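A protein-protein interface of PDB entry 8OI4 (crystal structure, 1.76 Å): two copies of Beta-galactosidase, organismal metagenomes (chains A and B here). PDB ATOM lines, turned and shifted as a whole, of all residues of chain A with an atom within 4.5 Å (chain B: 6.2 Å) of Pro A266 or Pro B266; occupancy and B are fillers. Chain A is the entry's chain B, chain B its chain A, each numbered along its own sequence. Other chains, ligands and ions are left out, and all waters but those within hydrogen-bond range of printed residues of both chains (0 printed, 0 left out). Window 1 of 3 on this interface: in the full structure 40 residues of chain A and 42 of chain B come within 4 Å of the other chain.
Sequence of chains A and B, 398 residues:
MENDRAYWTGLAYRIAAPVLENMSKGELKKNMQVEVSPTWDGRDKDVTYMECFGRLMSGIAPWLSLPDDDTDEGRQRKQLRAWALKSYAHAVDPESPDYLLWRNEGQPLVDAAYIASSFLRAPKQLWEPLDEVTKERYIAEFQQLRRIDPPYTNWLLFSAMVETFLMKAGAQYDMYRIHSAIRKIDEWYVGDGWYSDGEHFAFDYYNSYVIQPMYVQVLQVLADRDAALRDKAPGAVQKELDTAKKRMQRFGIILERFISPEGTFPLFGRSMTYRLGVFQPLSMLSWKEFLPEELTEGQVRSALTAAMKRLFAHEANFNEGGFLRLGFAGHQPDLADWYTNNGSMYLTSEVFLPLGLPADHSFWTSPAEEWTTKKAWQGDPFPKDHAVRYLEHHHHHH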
ATOM      1  N   TYR A 205      35.366  13.662  16.700  1.00  0.00           N
ATOM      2  CA  TYR A 205      35.214  12.796  17.848  1.00  0.00           C
ATOM      3  C   TYR A 205      36.479  12.056  18.270  1.00  0.00           C
ATOM      4  O   TYR A 205      36.391  11.100  19.040  1.00  0.00           O
ATOM      5  CB  TYR A 205      34.108  11.802  17.553  1.00  0.00           C
ATOM      6  CG  TYR A 205      32.692  12.362  17.634  1.00  0.00           C
ATOM      7  CD1 TYR A 205      32.118  12.664  18.855  1.00  0.00           C
ATOM      8  CD2 TYR A 205      31.918  12.518  16.493  1.00  0.00           C
ATOM      9  CE1 TYR A 205      30.792  13.115  18.947  1.00  0.00           C
ATOM     10  CE2 TYR A 205      30.605  12.986  16.566  1.00  0.00           C
ATOM     11  CZ  TYR A 205      30.045  13.278  17.805  1.00  0.00           C
ATOM     12  OH  TYR A 205      28.729  13.704  17.909  1.00  0.00           O
ATOM     13  N   ARG A 257      24.609  15.348  26.369  1.00  0.00           N
ATOM     14  CA  ARG A 257      23.784  16.395  25.792  1.00  0.00           C
ATOM     15  C   ARG A 257      23.729  16.401  24.264  1.00  0.00           C
ATOM     16  O   ARG A 257      22.932  17.131  23.684  1.00  0.00           O
ATOM     17  CB  ARG A 257      24.271  17.745  26.322  1.00  0.00           C
ATOM     18  CG  ARG A 257      23.723  18.002  27.725  1.00  0.00           C
ATOM     19  CD  ARG A 257      24.540  19.001  28.477  1.00  0.00           C
ATOM     20  NE  ARG A 257      23.913  19.356  29.745  1.00  0.00           N
ATOM     21  CZ  ARG A 257      22.966  20.273  29.896  1.00  0.00           C
ATOM     22  NH1 ARG A 257      22.487  20.964  28.867  1.00  0.00           N
ATOM     23  NH2 ARG A 257      22.514  20.531  31.122  1.00  0.00           N
ATOM     24  N   PHE A 258      24.599  15.598  23.634  1.00  0.00           N
ATOM     25  CA  PHE A 258      24.545  15.346  22.204  1.00  0.00           C
ATOM     26  C   PHE A 258      23.473  14.341  21.791  1.00  0.00           C
ATOM     27  O   PHE A 258      23.057  14.327  20.632  1.00  0.00           O
ATOM     28  CB  PHE A 258      25.901  14.829  21.713  1.00  0.00           C
ATOM     29  CG  PHE A 258      26.937  15.876  21.394  1.00  0.00           C
ATOM     30  CD1 PHE A 258      26.773  17.197  21.798  1.00  0.00           C
ATOM     31  CD2 PHE A 258      28.084  15.541  20.682  1.00  0.00           C
ATOM     32  CE1 PHE A 258      27.740  18.163  21.477  1.00  0.00           C
ATOM     33  CE2 PHE A 258      29.035  16.507  20.363  1.00  0.00           C
ATOM     34  CZ  PHE A 258      28.856  17.809  20.753  1.00  0.00           C
ATOM     35  N   PHE A 265      22.643  11.597  17.351  1.00  0.00           N
ATOM     36  CA  PHE A 265      23.669  12.515  17.813  1.00  0.00           C
ATOM     37  C   PHE A 265      24.282  13.203  16.606  1.00  0.00           C
ATOM     38  O   PHE A 265      24.044  12.804  15.480  1.00  0.00           O
ATOM     39  CB  PHE A 265      24.734  11.795  18.651  1.00  0.00           C
ATOM     40  CG  PHE A 265      25.244  10.494  18.075  1.00  0.00           C
ATOM     41  CD1 PHE A 265      24.575   9.295  18.315  1.00  0.00           C
ATOM     42  CD2 PHE A 265      26.365  10.470  17.263  1.00  0.00           C
ATOM     43  CE1 PHE A 265      25.036   8.100  17.799  1.00  0.00           C
ATOM     44  CE2 PHE A 265      26.836   9.267  16.739  1.00  0.00           C
ATOM     45  CZ  PHE A 265      26.167   8.080  17.008  1.00  0.00           C
ATOM     46  N   PRO A 266      25.011  14.319  16.787  1.00  0.00           N
ATOM     47  CA  PRO A 266      25.578  15.047  15.651  1.00  0.00           C
ATOM     48  C   PRO A 266      26.643  14.229  14.926  1.00  0.00           C
ATOM     49  O   PRO A 266      27.379  13.456  15.542  1.00  0.00           O
ATOM     50  CB  PRO A 266      26.153  16.309  16.304  1.00  0.00           C
ATOM     51  CG  PRO A 266      25.468  16.405  17.646  1.00  0.00           C
ATOM     52  CD  PRO A 266      25.275  14.990  18.068  1.00  0.00           C
ATOM     53  N   LEU A 267      26.692  14.409  13.611  1.00  0.00           N
ATOM     54  CA  LEU A 267      27.663  13.743  12.758  1.00  0.00           C
ATOM     55  C   LEU A 267      28.606  14.806  12.195  1.00  0.00           C
ATOM     56  O   LEU A 267      28.216  15.600  11.346  1.00  0.00           O
ATOM     57  CB  LEU A 267      26.927  13.021  11.650  1.00  0.00           C
ATOM     58  CG  LEU A 267      25.892  12.045  12.120  1.00  0.00           C
ATOM     59  CD1 LEU A 267      25.186  11.438  10.963  1.00  0.00           C
ATOM     60  CD2 LEU A 267      26.527  10.947  12.955  1.00  0.00           C
ATOM     61  N   PHE A 268      29.845  14.804  12.678  1.00  0.00           N
ATOM     62  CA  PHE A 268      30.812  15.791  12.247  1.00  0.00           C
ATOM     63  C   PHE A 268      32.204  15.194  12.396  1.00  0.00           C
ATOM     64  O   PHE A 268      32.416  14.259  13.162  1.00  0.00           O
ATOM     65  CB  PHE A 268      30.648  17.118  13.029  1.00  0.00           C
ATOM     66  CG  PHE A 268      30.837  16.970  14.504  1.00  0.00           C
ATOM     67  CD1 PHE A 268      32.101  16.963  15.060  1.00  0.00           C
ATOM     68  CD2 PHE A 268      29.752  16.800  15.342  1.00  0.00           C
ATOM     69  CE1 PHE A 268      32.283  16.793  16.432  1.00  0.00           C
ATOM     70  CE2 PHE A 268      29.933  16.641  16.715  1.00  0.00           C
ATOM     71  CZ  PHE A 268      31.208  16.621  17.250  1.00  0.00           C
ATOM     72  N   TYR B 205      26.887  28.228  22.585  1.00  0.00           N
ATOM     73  CA  TYR B 205      26.408  28.782  21.338  1.00  0.00           C
ATOM     74  C   TYR B 205      26.607  30.292  21.199  1.00  0.00           C
ATOM     75  O   TYR B 205      26.004  30.900  20.322  1.00  0.00           O
ATOM     76  CB  TYR B 205      24.933  28.445  21.198  1.00  0.00           C
ATOM     77  CG  TYR B 205      24.635  26.996  20.831  1.00  0.00           C
ATOM     78  CD1 TYR B 205      24.883  26.517  19.553  1.00  0.00           C
ATOM     79  CD2 TYR B 205      24.010  26.144  21.733  1.00  0.00           C
ATOM     80  CE1 TYR B 205      24.536  25.214  19.184  1.00  0.00           C
ATOM     81  CE2 TYR B 205      23.678  24.828  21.387  1.00  0.00           C
ATOM     82  CZ  TYR B 205      23.924  24.374  20.098  1.00  0.00           C
ATOM     83  OH  TYR B 205      23.568  23.092  19.729  1.00  0.00           O
ATOM     84  N   ILE B 254      28.816  22.785  10.587  1.00  0.00           N
ATOM     85  CA  ILE B 254      28.679  22.152  11.886  1.00  0.00           C
ATOM     86  C   ILE B 254      27.254  22.275  12.417  1.00  0.00           C
ATOM     87  O   ILE B 254      26.671  21.285  12.857  1.00  0.00           O
ATOM     88  CB  ILE B 254      29.734  22.724  12.880  1.00  0.00           C
ATOM     89  CG1 ILE B 254      31.156  22.331  12.456  1.00  0.00           C
ATOM     90  CG2 ILE B 254      29.436  22.316  14.315  1.00  0.00           C
ATOM     91  CD1 ILE B 254      32.221  23.127  13.128  1.00  0.00           C
ATOM     92  N   ARG B 257      24.837  19.946  10.804  1.00  0.00           N
ATOM     93  CA  ARG B 257      25.069  18.588  11.276  1.00  0.00           C
ATOM     94  C   ARG B 257      24.642  18.351  12.727  1.00  0.00           C
ATOM     95  O   ARG B 257      24.618  17.211  13.177  1.00  0.00           O
ATOM     96  CB  ARG B 257      26.540  18.240  11.087  1.00  0.00           C
ATOM     97  CG  ARG B 257      26.833  17.866   9.636  1.00  0.00           C
ATOM     98  CD  ARG B 257      28.286  18.014   9.300  1.00  0.00           C
ATOM     99  NE  ARG B 257      28.581  17.469   7.979  1.00  0.00           N
ATOM    100  CZ  ARG B 257      28.814  16.197   7.703  1.00  0.00           C
ATOM    101  NH1 ARG B 257      28.816  15.261   8.644  1.00  0.00           N
ATOM    102  NH2 ARG B 257      29.084  15.855   6.452  1.00  0.00           N
ATOM    103  N   PHE B 258      24.325  19.434  13.445  1.00  0.00           N
ATOM    104  CA  PHE B 258      23.719  19.353  14.770  1.00  0.00           C
ATOM    105  C   PHE B 258      22.225  19.042  14.759  1.00  0.00           C
ATOM    106  O   PHE B 258      21.684  18.585  15.753  1.00  0.00           O
ATOM    107  CB  PHE B 258      23.932  20.674  15.516  1.00  0.00           C
ATOM    108  CG  PHE B 258      25.243  20.832  16.240  1.00  0.00           C
ATOM    109  CD1 PHE B 258      26.318  19.980  15.983  1.00  0.00           C
ATOM    110  CD2 PHE B 258      25.421  21.853  17.160  1.00  0.00           C
ATOM    111  CE1 PHE B 258      27.530  20.130  16.675  1.00  0.00           C
ATOM    112  CE2 PHE B 258      26.632  22.002  17.842  1.00  0.00           C
ATOM    113  CZ  PHE B 258      27.665  21.128  17.614  1.00  0.00           C
ATOM    114  N   ILE B 259      21.559  19.305  13.634  1.00  0.00           N
ATOM    115  CA  ILE B 259      20.124  19.094  13.554  1.00  0.00           C
ATOM    116  C   ILE B 259      19.859  17.604  13.342  1.00  0.00           C
ATOM    117  O   ILE B 259      20.343  16.999  12.385  1.00  0.00           O
ATOM    118  CB  ILE B 259      19.469  19.993  12.485  1.00  0.00           C
ATOM    119  CG1 ILE B 259      19.817  21.480  12.771  1.00  0.00           C
ATOM    120  CG2 ILE B 259      17.991  19.743  12.422  1.00  0.00           C
ATOM    121  CD1 ILE B 259      19.397  22.449  11.704  1.00  0.00           C
ATOM    122  N   THR B 264      15.697  18.131  16.335  1.00  0.00           N
ATOM    123  CA  THR B 264      16.285  18.609  17.573  1.00  0.00           C
ATOM    124  C   THR B 264      17.760  18.935  17.342  1.00  0.00           C
ATOM    125  O   THR B 264      18.272  18.814  16.235  1.00  0.00           O
ATOM    126  CB  THR B 264      16.072  17.606  18.705  1.00  0.00           C
ATOM    127  OG1 THR B 264      16.936  16.468  18.528  1.00  0.00           O
ATOM    128  CG2 THR B 264      14.625  17.150  18.802  1.00  0.00           C
ATOM    129  N   PHE B 265      18.421  19.392  18.405  1.00  0.00           N
ATOM    130  CA  PHE B 265      19.824  19.732  18.359  1.00  0.00           C
ATOM    131  C   PHE B 265      20.395  19.650  19.768  1.00  0.00           C
ATOM    132  O   PHE B 265      19.649  19.560  20.736  1.00  0.00           O
ATOM    133  CB  PHE B 265      20.028  21.117  17.741  1.00  0.00           C
ATOM    134  CG  PHE B 265      19.130  22.205  18.261  1.00  0.00           C
ATOM    135  CD1 PHE B 265      17.890  22.428  17.695  1.00  0.00           C
ATOM    136  CD2 PHE B 265      19.538  23.015  19.315  1.00  0.00           C
ATOM    137  CE1 PHE B 265      17.072  23.464  18.158  1.00  0.00           C
ATOM    138  CE2 PHE B 265      18.716  24.038  19.785  1.00  0.00           C
ATOM    139  CZ  PHE B 265      17.490  24.260  19.199  1.00  0.00           C
ATOM    140  N   PRO B 266      21.735  19.628  19.934  1.00  0.00           N
ATOM    141  CA  PRO B 266      22.331  19.503  21.260  1.00  0.00           C
ATOM    142  C   PRO B 266      22.066  20.734  22.123  1.00  0.00           C
ATOM    143  O   PRO B 266      21.991  21.851  21.624  1.00  0.00           O
ATOM    144  CB  PRO B 266      23.807  19.300  20.947  1.00  0.00           C
ATOM    145  CG  PRO B 266      23.860  18.889  19.538  1.00  0.00           C
ATOM    146  CD  PRO B 266      22.744  19.615  18.870  1.00  0.00           C
ATOM    147  N   LEU B 267      21.907  20.484  23.421  1.00  0.00           N
ATOM    148  CA  LEU B 267      21.684  21.515  24.417  1.00  0.00           C
ATOM    149  C   LEU B 267      22.898  21.543  25.336  1.00  0.00           C
ATOM    150  O   LEU B 267      23.088  20.651  26.152  1.00  0.00           O
ATOM    151  CB  LEU B 267      20.417  21.182  25.187  1.00  0.00           C
ATOM    152  CG  LEU B 267      19.186  21.018  24.320  1.00  0.00           C
ATOM    153  CD1 LEU B 267      18.032  20.623  25.127  1.00  0.00           C
ATOM    154  CD2 LEU B 267      18.893  22.281  23.572  1.00  0.00           C
ATOM    155  N   PHE B 268      23.707  22.595  25.202  1.00  0.00           N
ATOM    156  CA  PHE B 268      24.913  22.725  25.990  1.00  0.00           C
ATOM    157  C   PHE B 268      25.228  24.211  26.110  1.00  0.00           C
ATOM    158  O   PHE B 268      24.786  25.023  25.299  1.00  0.00           O
ATOM    159  CB  PHE B 268      26.076  21.915  25.361  1.00  0.00           C
ATOM    160  CG  PHE B 268      26.446  22.353  23.977  1.00  0.00           C
ATOM    161  CD1 PHE B 268      27.277  23.443  23.775  1.00  0.00           C
ATOM    162  CD2 PHE B 268      25.921  21.722  22.869  1.00  0.00           C
ATOM    163  CE1 PHE B 268      27.591  23.885  22.487  1.00  0.00           C
ATOM    164  CE2 PHE B 268      26.250  22.152  21.581  1.00  0.00           C
ATOM    165  CZ  PHE B 268      27.079  23.246  21.402  1.00  0.00           C
ATOM    166  N   MET B 272      20.775  28.732  27.087  1.00  0.00           N
ATOM    167  CA  MET B 272      20.031  27.804  26.251  1.00  0.00           C
ATOM    168  C   MET B 272      18.591  28.267  26.022  1.00  0.00           C
ATOM    169  O   MET B 272      17.918  27.779  25.121  1.00  0.00           O
ATOM    170  CB  MET B 272      20.109  26.403  26.885  1.00  0.00           C
ATOM    171  CG  MET B 272      20.213  25.266  25.888  1.00  0.00           C
ATOM    172  SD  MET B 272      21.381  25.460  24.532  1.00  0.00           S
ATOM    173  CE  MET B 272      20.234  25.755  23.212  1.00  0.00           C
ATOM    174  N   VAL B 278      20.527  29.883  18.233  1.00  0.00           N
ATOM    175  CA  VAL B 278      21.674  29.030  17.942  1.00  0.00           C
ATOM    176  C   VAL B 278      21.986  28.934  16.448  1.00  0.00           C
ATOM    177  O   VAL B 278      23.102  28.598  16.067  1.00  0.00           O
ATOM    178  CB  VAL B 278      21.504  27.610  18.536  1.00  0.00           C
ATOM    179  CG1 VAL B 278      21.250  27.654  20.023  1.00  0.00           C
ATOM    180  CG2 VAL B 278      20.426  26.836  17.823  1.00  0.00           C
ATOM    181  N   THR B 373      21.951  14.397   8.989  1.00  0.00           N
ATOM    182  CA  THR B 373      21.633  13.316   9.924  1.00  0.00           C
ATOM    183  C   THR B 373      20.414  12.522   9.469  1.00  0.00           C
ATOM    184  O   THR B 373      20.311  11.318   9.725  1.00  0.00           O
ATOM    185  CB  THR B 373      21.385  13.827  11.346  1.00  0.00           C
ATOM    186  OG1 THR B 373      20.230  14.653  11.332  1.00  0.00           O
ATOM    187  CG2 THR B 373      22.603  14.543  11.924  1.00  0.00           C
ATOM    188  N   TRP B 377      20.737   8.468   9.232  1.00  0.00           N
ATOM    189  CA  TRP B 377      19.945   7.505   9.976  1.00  0.00           C
ATOM    190  C   TRP B 377      18.931   6.719   9.148  1.00  0.00           C
ATOM    191  O   TRP B 377      18.420   5.703   9.629  1.00  0.00           O
ATOM    192  CB  TRP B 377      19.271   8.166  11.203  1.00  0.00           C
ATOM    193  CG  TRP B 377      20.059   7.918  12.451  1.00  0.00           C
ATOM    194  CD1 TRP B 377      20.018   6.800  13.228  1.00  0.00           C
ATOM    195  CD2 TRP B 377      21.112   8.726  12.969  1.00  0.00           C
ATOM    196  NE1 TRP B 377      20.932   6.896  14.239  1.00  0.00           N
ATOM    197  CE2 TRP B 377      21.616   8.074  14.110  1.00  0.00           C
ATOM    198  CE3 TRP B 377      21.636   9.971  12.624  1.00  0.00           C
ATOM    199  CZ2 TRP B 377      22.658   8.600  14.866  1.00  0.00           C
ATOM    200  CZ3 TRP B 377      22.648  10.503  13.393  1.00  0.00           C
ATOM    201  CH2 TRP B 377      23.152   9.819  14.492  1.00  0.00           C
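The backbone carbonyl oxygen (O) of Leu B267 is in hydrogen-bond range of the guanidinium group (NH1) of Arg A257, at 2.8 Å.
The guanidinium group (NH1) of Arg B257 lies within hydrogen-bond range of the backbone carbonyl oxygen (O) of Leu A267, 2.8 Å away.
Arg A257 touches Pro B266, and with the chains exchanged Pro A266 touches Arg B257.
Arg A257 touches Leu B267, and with the chains exchanged Leu A267 touches Arg B257.
Phe A258 touches Pro B266, and with the chains exchanged Pro A266 touches Phe B258.
Pro B266 touches its own counterpart, Pro A266.
7 positions are printed for both chains.
Printed residues of chain B that touch a printed residue of chain A: Arg B257, Phe B258, Pro B266, Leu B267 and Trp B377.
Hydrophobic or aromatic side chains of chain B within 4 Å of the printed part of chain A: Phe B258, Pro B266 and Trp B377.
Among the printed residues, no Asp or Glu carboxylate lies within 4 Å of a Lys or Arg side-chain nitrogen of the other chain.
OH of Tyr B205 sits at hydrogen-bond distance from O of Pro B266 (2.8 Å).
The side-chain hydroxyl (OH) of Tyr A205 is in hydrogen-bond range of the backbone carbonyl oxygen (O) of Pro A266 (2.7 Å).
Of the printed residues of chain B, Arg A257 touches Pro B266 and Leu B267.
Printed residues of chain B within 4 Å of Phe A265: Trp B377.
Printed residues of chain B within 4 Å of Pro A266: Arg B257, Phe B258 and Pro B266.
Printed residues of chain A within 4 Å of Phe B258: Pro A266 (3.7 Å).
Pro B266 touches just these residues of chain A: Arg A257, Phe A258 and Pro A266.
The nearest printed residue of chain A that does not touch Pro B266 is Phe A265 (6.4 Å).
The nearest printed residue of chain A that does not touch Arg B257 is Phe A268 (4.2 Å).
Pro B266 touches Arg A257 (CA to O, 3.4 Å).
Phe A258 touches Pro B266.
Phe A265 touches Trp B377.
CA of Pro A266 touches O of Arg B257, at 3.4 Å.
Pro A266 touches Phe B258 (CB to CD1, 3.7 Å).
CG of Pro B266 touches CG of Pro A266, at 3.5 Å.
Trp B377 touches Leu A267.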
